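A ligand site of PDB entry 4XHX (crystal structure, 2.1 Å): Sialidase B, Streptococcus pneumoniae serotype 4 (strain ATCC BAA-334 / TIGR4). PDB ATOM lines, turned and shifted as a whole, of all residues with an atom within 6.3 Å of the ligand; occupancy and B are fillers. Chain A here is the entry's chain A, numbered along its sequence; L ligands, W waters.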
ATOM      1  N   LEU A 211     -29.654  14.355  27.476  1.00  0.00           N
ATOM      2  CA  LEU A 211     -28.557  13.399  27.292  1.00  0.00           C
ATOM      3  C   LEU A 211     -29.065  12.238  26.487  1.00  0.00           C
ATOM      4  O   LEU A 211     -30.202  11.782  26.696  1.00  0.00           O
ATOM      5  CB  LEU A 211     -28.034  12.850  28.631  1.00  0.00           C
ATOM      6  CG  LEU A 211     -27.175  13.730  29.519  1.00  0.00           C
ATOM      7  CD1 LEU A 211     -27.003  13.059  30.864  1.00  0.00           C
ATOM      8  CD2 LEU A 211     -25.817  14.011  28.878  1.00  0.00           C
ATOM      9  N   TYR A 212     -28.226  11.754  25.566  1.00  0.00           N
ATOM     10  CA  TYR A 212     -28.564  10.624  24.706  1.00  0.00           C
ATOM     11  C   TYR A 212     -27.308   9.831  24.303  1.00  0.00           C
ATOM     12  O   TYR A 212     -26.308  10.406  23.856  1.00  0.00           O
ATOM     13  CB  TYR A 212     -29.341  11.119  23.469  1.00  0.00           C
ATOM     14  CG  TYR A 212     -30.069  10.033  22.693  1.00  0.00           C
ATOM     15  CD1 TYR A 212     -29.372   9.167  21.856  1.00  0.00           C
ATOM     16  CD2 TYR A 212     -31.452   9.880  22.784  1.00  0.00           C
ATOM     17  CE1 TYR A 212     -30.030   8.188  21.130  1.00  0.00           C
ATOM     18  CE2 TYR A 212     -32.124   8.894  22.066  1.00  0.00           C
ATOM     19  CZ  TYR A 212     -31.399   8.057  21.240  1.00  0.00           C
ATOM     20  OH  TYR A 212     -32.051   7.065  20.517  1.00  0.00           O
ATOM     21  N   THR A 213     -27.377   8.505  24.443  1.00  0.00           N
ATOM     22  CA  THR A 213     -26.226   7.654  24.137  1.00  0.00           C
ATOM     23  C   THR A 213     -26.314   7.082  22.709  1.00  0.00           C
ATOM     24  O   THR A 213     -27.207   6.304  22.385  1.00  0.00           O
ATOM     25  CB  THR A 213     -26.096   6.513  25.172  1.00  0.00           C
ATOM     26  OG1 THR A 213     -26.058   7.071  26.496  1.00  0.00           O
ATOM     27  CG2 THR A 213     -24.824   5.654  24.910  1.00  0.00           C
ATOM     28  N   LEU A 214     -25.362   7.475  21.856  1.00  0.00           N
ATOM     29  CA  LEU A 214     -25.389   7.092  20.458  1.00  0.00           C
ATOM     30  C   LEU A 214     -24.759   5.715  20.224  1.00  0.00           C
ATOM     31  O   LEU A 214     -23.984   5.230  21.059  1.00  0.00           O
ATOM     32  CB  LEU A 214     -24.654   8.153  19.616  1.00  0.00           C
ATOM     33  CG  LEU A 214     -25.186   9.582  19.747  1.00  0.00           C
ATOM     34  CD1 LEU A 214     -24.300  10.543  18.949  1.00  0.00           C
ATOM     35  CD2 LEU A 214     -26.646   9.643  19.286  1.00  0.00           C
ATOM     36  N   GLN A 456     -35.257  13.140  25.595  1.00  0.00           N
ATOM     37  CA  GLN A 456     -34.997  12.154  24.543  1.00  0.00           C
ATOM     38  C   GLN A 456     -36.246  11.797  23.758  1.00  0.00           C
ATOM     39  O   GLN A 456     -37.353  11.696  24.324  1.00  0.00           O
ATOM     40  CB  GLN A 456     -34.436  10.871  25.131  1.00  0.00           C
ATOM     41  CG  GLN A 456     -33.289  11.027  26.116  1.00  0.00           C
ATOM     42  CD  GLN A 456     -32.756   9.666  26.557  1.00  0.00           C
ATOM     43  OE1 GLN A 456     -33.468   8.648  26.459  1.00  0.00           O
ATOM     44  NE2 GLN A 456     -31.523   9.633  27.047  1.00  0.00           N
ATOM     45  N   GLY A 457     -36.086  11.606  22.455  1.00  0.00           N
ATOM     46  CA  GLY A 457     -37.096  10.915  21.681  1.00  0.00           C
ATOM     47  C   GLY A 457     -36.844   9.427  21.873  1.00  0.00           C
ATOM     48  O   GLY A 457     -35.915   9.043  22.594  1.00  0.00           O
ATOM     49  N   LEU A 458     -37.660   8.587  21.243  1.00  0.00           N
ATOM     50  CA  LEU A 458     -37.494   7.150  21.376  1.00  0.00           C
ATOM     51  C   LEU A 458     -37.298   6.489  20.011  1.00  0.00           C
ATOM     52  O   LEU A 458     -38.069   6.712  19.069  1.00  0.00           O
ATOM     53  CB  LEU A 458     -38.697   6.534  22.094  1.00  0.00           C
ATOM     54  CG  LEU A 458     -38.785   5.004  22.178  1.00  0.00           C
ATOM     55  CD1 LEU A 458     -37.662   4.431  23.023  1.00  0.00           C
ATOM     56  CD2 LEU A 458     -40.140   4.563  22.746  1.00  0.00           C
ATOM     57  N   ALA A 459     -36.231   5.711  19.902  1.00  0.00           N
ATOM     58  CA  ALA A 459     -35.947   4.895  18.719  1.00  0.00           C
ATOM     59  C   ALA A 459     -36.282   3.477  19.114  1.00  0.00           C
ATOM     60  O   ALA A 459     -35.626   2.906  19.971  1.00  0.00           O
ATOM     61  CB  ALA A 459     -34.451   4.991  18.326  1.00  0.00           C
ATOM     62  N   LYS A 461     -36.387  -0.386  19.327  1.00  0.00           N
ATOM     63  CA  LYS A 461     -35.304  -1.349  19.151  1.00  0.00           C
ATOM     64  C   LYS A 461     -35.478  -2.212  17.897  1.00  0.00           C
ATOM     65  O   LYS A 461     -34.538  -2.394  17.115  1.00  0.00           O
ATOM     66  CB  LYS A 461     -35.234  -2.259  20.372  1.00  0.00           C
ATOM     67  CG  LYS A 461     -35.099  -1.544  21.711  1.00  0.00           C
ATOM     68  CD  LYS A 461     -33.685  -1.084  21.989  1.00  0.00           C
ATOM     69  CE  LYS A 461     -33.418  -0.986  23.494  1.00  0.00           C
ATOM     70  NZ  LYS A 461     -34.330  -0.024  24.194  1.00  0.00           N
ATOM     71  N   ALA A 557     -36.424   9.568  32.096  1.00  0.00           N
ATOM     72  CA  ALA A 557     -36.639   8.135  32.305  1.00  0.00           C
ATOM     73  C   ALA A 557     -35.922   7.264  31.290  1.00  0.00           C
ATOM     74  O   ALA A 557     -35.938   7.547  30.083  1.00  0.00           O
ATOM     75  CB  ALA A 557     -38.133   7.821  32.299  1.00  0.00           C
ATOM     76  N   ILE A 558     -35.259   6.213  31.773  1.00  0.00           N
ATOM     77  CA  ILE A 558     -34.624   5.260  30.874  1.00  0.00           C
ATOM     78  C   ILE A 558     -34.945   3.825  31.267  1.00  0.00           C
ATOM     79  O   ILE A 558     -35.282   3.536  32.410  1.00  0.00           O
ATOM     80  CB  ILE A 558     -33.106   5.404  30.892  1.00  0.00           C
ATOM     81  CG1 ILE A 558     -32.596   5.280  32.333  1.00  0.00           C
ATOM     82  CG2 ILE A 558     -32.692   6.710  30.227  1.00  0.00           C
ATOM     83  CD1 ILE A 558     -31.114   5.083  32.466  1.00  0.00           C
ATOM     84  N   LYS A 559     -34.836   2.941  30.280  1.00  0.00           N
ATOM     85  CA  LYS A 559     -34.875   1.509  30.500  1.00  0.00           C
ATOM     86  C   LYS A 559     -33.431   1.019  30.539  1.00  0.00           C
ATOM     87  O   LYS A 559     -32.729   1.098  29.526  1.00  0.00           O
ATOM     88  CB  LYS A 559     -35.660   0.845  29.374  1.00  0.00           C
ATOM     89  CG  LYS A 559     -35.459  -0.667  29.257  1.00  0.00           C
ATOM     90  CD  LYS A 559     -36.114  -1.401  30.392  1.00  0.00           C
ATOM     91  CE  LYS A 559     -36.338  -2.872  30.027  1.00  0.00           C
ATOM     92  NZ  LYS A 559     -35.070  -3.542  29.611  1.00  0.00           N
ATOM     93  N   SER A 561     -30.075  -1.339  30.586  1.00  0.00           N
ATOM     94  CA  SER A 561     -29.762  -2.475  29.721  1.00  0.00           C
ATOM     95  C   SER A 561     -29.546  -3.796  30.467  1.00  0.00           C
ATOM     96  O   SER A 561     -29.722  -4.874  29.885  1.00  0.00           O
ATOM     97  CB  SER A 561     -28.526  -2.191  28.847  1.00  0.00           C
ATOM     98  OG  SER A 561     -27.330  -2.440  29.587  1.00  0.00           O
ATOM     99  N   ILE A 618     -31.081  11.922  31.927  1.00  0.00           N
ATOM    100  CA  ILE A 618     -30.332  10.727  32.296  1.00  0.00           C
ATOM    101  C   ILE A 618     -30.109   9.836  31.102  1.00  0.00           C
ATOM    102  O   ILE A 618     -30.973   9.696  30.232  1.00  0.00           O
ATOM    103  CB  ILE A 618     -31.007   9.911  33.428  1.00  0.00           C
ATOM    104  CG1 ILE A 618     -32.452   9.559  33.045  1.00  0.00           C
ATOM    105  CG2 ILE A 618     -30.993  10.686  34.728  1.00  0.00           C
ATOM    106  CD1 ILE A 618     -33.084   8.644  34.011  1.00  0.00           C
ATOM    107  N   THR A 619     -28.946   9.203  31.064  1.00  0.00           N
ATOM    108  CA  THR A 619     -28.693   8.207  30.057  1.00  0.00           C
ATOM    109  C   THR A 619     -27.761   7.130  30.617  1.00  0.00           C
ATOM    110  O   THR A 619     -26.927   7.390  31.498  1.00  0.00           O
ATOM    111  CB  THR A 619     -28.136   8.839  28.756  1.00  0.00           C
ATOM    112  OG1 THR A 619     -28.252   7.909  27.667  1.00  0.00           O
ATOM    113  CG2 THR A 619     -26.679   9.258  28.932  1.00  0.00           C
ATOM    114  N   GLU A 620     -27.934   5.905  30.119  1.00  0.00           N
ATOM    115  CA  GLU A 620     -26.975   4.865  30.420  1.00  0.00           C
ATOM    116  C   GLU A 620     -25.737   5.062  29.538  1.00  0.00           C
ATOM    117  O   GLU A 620     -25.826   5.067  28.317  1.00  0.00           O
ATOM    118  CB  GLU A 620     -27.589   3.478  30.201  1.00  0.00           C
ATOM    119  CG  GLU A 620     -26.607   2.336  30.414  1.00  0.00           C
ATOM    120  CD  GLU A 620     -27.271   0.974  30.349  1.00  0.00           C
ATOM    121  OE1 GLU A 620     -28.508   0.911  30.198  1.00  0.00           O
ATOM    122  OE2 GLU A 620     -26.553  -0.051  30.456  1.00  0.00           O
ATOM    123  N   LEU A 621     -24.584   5.235  30.167  1.00  0.00           N
ATOM    124  CA  LEU A 621     -23.338   5.392  29.409  1.00  0.00           C
ATOM    125  C   LEU A 621     -22.936   4.024  28.857  1.00  0.00           C
ATOM    126  O   LEU A 621     -23.341   2.998  29.393  1.00  0.00           O
ATOM    127  CB  LEU A 621     -22.255   5.972  30.311  1.00  0.00           C
ATOM    128  CG  LEU A 621     -22.664   7.321  30.939  1.00  0.00           C
ATOM    129  CD1 LEU A 621     -21.747   7.731  32.080  1.00  0.00           C
ATOM    130  CD2 LEU A 621     -22.694   8.425  29.884  1.00  0.00           C
ATOM    131  N   PRO A 622     -22.162   4.002  27.768  1.00  0.00           N
ATOM    132  CA  PRO A 622     -21.754   2.713  27.179  1.00  0.00           C
ATOM    133  C   PRO A 622     -21.146   1.706  28.174  1.00  0.00           C
ATOM    134  O   PRO A 622     -21.268   0.506  27.961  1.00  0.00           O
ATOM    135  CB  PRO A 622     -20.704   3.120  26.137  1.00  0.00           C
ATOM    136  CG  PRO A 622     -21.153   4.501  25.698  1.00  0.00           C
ATOM    137  CD  PRO A 622     -21.845   5.142  26.883  1.00  0.00           C
ATOM    138  N   ASN A 623     -20.513   2.183  29.233  1.00  0.00           N
ATOM    139  CA  ASN A 623     -19.872   1.300  30.203  1.00  0.00           C
ATOM    140  C   ASN A 623     -20.843   0.815  31.282  1.00  0.00           C
ATOM    141  O   ASN A 623     -20.432   0.133  32.231  1.00  0.00           O
ATOM    142  CB  ASN A 623     -18.679   1.992  30.870  1.00  0.00           C
ATOM    143  CG  ASN A 623     -19.073   3.299  31.567  1.00  0.00           C
ATOM    144  OD1 ASN A 623     -20.267   3.659  31.608  1.00  0.00           O
ATOM    145  ND2 ASN A 623     -18.092   3.997  32.137  1.00  0.00           N
ATOM    146  N   HIS A 624     -22.116   1.208  31.142  1.00  0.00           N
ATOM    147  CA  HIS A 624     -23.210   0.860  32.050  1.00  0.00           C
ATOM    148  C   HIS A 624     -23.283   1.724  33.310  1.00  0.00           C
ATOM    149  O   HIS A 624     -24.081   1.435  34.197  1.00  0.00           O
ATOM    150  CB  HIS A 624     -23.261  -0.639  32.370  1.00  0.00           C
ATOM    151  CG  HIS A 624     -23.252  -1.515  31.154  1.00  0.00           C
ATOM    152  ND1 HIS A 624     -24.205  -1.417  30.160  1.00  0.00           N
ATOM    153  CD2 HIS A 624     -22.396  -2.495  30.756  1.00  0.00           C
ATOM    154  CE1 HIS A 624     -23.940  -2.290  29.205  1.00  0.00           C
ATOM    155  NE2 HIS A 624     -22.845  -2.955  29.550  1.00  0.00           N
HETATM  156  C1  LIG L   1     -25.527   0.679  26.644  1.00  0.00           C
HETATM  157  C2  LIG L   1     -25.994  -0.018  25.419  1.00  0.00           C
HETATM  158  C3  LIG L   1     -25.764   2.151  26.557  1.00  0.00           C
HETATM  159  C4  LIG L   1     -27.402   0.339  25.027  1.00  0.00           C
HETATM  160  C5  LIG L   1     -27.186   2.504  26.147  1.00  0.00           C
HETATM  161  C6  LIG L   1     -29.205   3.558  24.242  1.00  0.00           C
HETATM  162  C7  LIG L   1     -31.244   4.358  25.417  1.00  0.00           C
HETATM  163  C8  LIG L   1     -30.564   5.596  23.513  1.00  0.00           C
HETATM  164  C9  LIG L   1     -31.839   5.719  25.398  1.00  0.00           C
HETATM  165  C10 LIG L   1     -30.886   6.507  24.661  1.00  0.00           C
HETATM  166  C11 LIG L   1     -27.611   1.827  24.900  1.00  0.00           C
HETATM  167  C12 LIG L   1     -30.610   4.199  24.094  1.00  0.00           C
HETATM  168  N1  LIG L   1     -29.038   2.115  24.619  1.00  0.00           N
HETATM  169  O1  LIG L   1     -31.738   1.803  23.793  1.00  0.00           O
HETATM  170  O2  LIG L   1     -32.989   3.706  23.145  1.00  0.00           O
HETATM  171  O3  LIG L   1     -31.969   6.215  26.685  1.00  0.00           O
HETATM  172  O4  LIG L   1     -29.755   6.736  25.431  1.00  0.00           O
HETATM  173  O5  LIG L   1     -31.207   3.022  21.811  1.00  0.00           O
HETATM  174  S1  LIG L   1     -31.678   3.146  23.166  1.00  0.00           S
HETATM  175  O   HOH W   1     -30.231   5.039  28.597  1.00  0.00           O
HETATM  176  O   HOH W   2     -34.099   5.929  21.859  1.00  0.00           O
HETATM  177  O   HOH W   3     -33.493   1.625  26.377  1.00  0.00           O
HETATM  178  O   HOH W   4     -34.195   4.184  27.709  1.00  0.00           O
HETATM  179  O   HOH W   5     -30.815   4.884  19.883  1.00  0.00           O
HETATM  180  O   HOH W   6     -29.535   0.727  21.889  1.00  0.00           O
HETATM  181  O   HOH W   7     -22.439  -0.283  25.522  1.00  0.00           O
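Tyr 212 touches the ligand. Ile 558 touches the ligand (CG2 to O3, 3.6 Å). O of Glu 620 touches C3 of the ligand, 3.4 Å away. O of Leu 621 touches C3 of the ligand, at 3.8 Å. Hydrophobic or aromatic side chains that line the ligand: Tyr 212 and Ile 558. Of the 20 residues printed, 8 come within 4 Å of the ligand. The nearest printed residue that does not touch the ligand is Pro 622 (4.1 Å).
Water W5 bridges OH of Tyr 212 (2.6 Å) and O5 of the ligand (2.7 Å). Water W2 lies within hydrogen-bond range of OH of Tyr 212 (2.7 Å), O2 of the ligand (2.8 Å) and N of Ala 459 (2.9 Å). Water W1 bridges an oxygen (O3) of the ligand and the backbone NH of Glu 620. Water W3 lies within hydrogen-bond range of the side-chain amino group of Lys 461 (2.9 Å), an oxygen (O1) of the ligand (3.1 Å) and the backbone carbonyl oxygen of Lys 559 (3.3 Å). Water W4 lies within hydrogen-bond range of the backbone NH (N) of Lys 559 (2.9 Å) and an oxygen (O3) of the ligand (3.2 Å).
N of Thr 213 is in hydrogen-bond range of O4 of the ligand, at 3.1 Å. The side-chain amide oxygen (OE1) of Gln 456 lies within hydrogen-bond range of an oxygen (O3) of the ligand (2.9 Å). The side-chain hydroxyl (OG1) of Thr 619 is in hydrogen-bond range of an oxygen (O4) of the ligand (2.9 Å). An oxygen (O1) of the ligand lies within salt-bridge range of the side-chain amino group (NZ) of Lys 461 (3.2 Å).
The side-chain amide nitrogen (NE2) of Gln 456 lies within hydrogen-bond range of the backbone carbonyl oxygen (O) of Leu 211, 2.5 Å away. The side-chain hydroxyl of Thr 213 sits at hydrogen-bond distance from the backbone carbonyl oxygen of Glu 620, at 2.7 Å. O of Ile 618 lies within hydrogen-bond range of NE2 of Gln 456 (3.2 Å). OE2 of Glu 620 is in hydrogen-bond range of ND1 of His 624, at 2.7 Å. The side-chain hydroxyl (OG1) of Thr 619 is in hydrogen-bond range of the side-chain hydroxyl (OG1) of Thr 213 (2.6 Å). The side-chain hydroxyl (OG) of Ser 561 is in hydrogen-bond range of the side-chain carboxylate (OE2) of Glu 620, at 2.7 Å.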
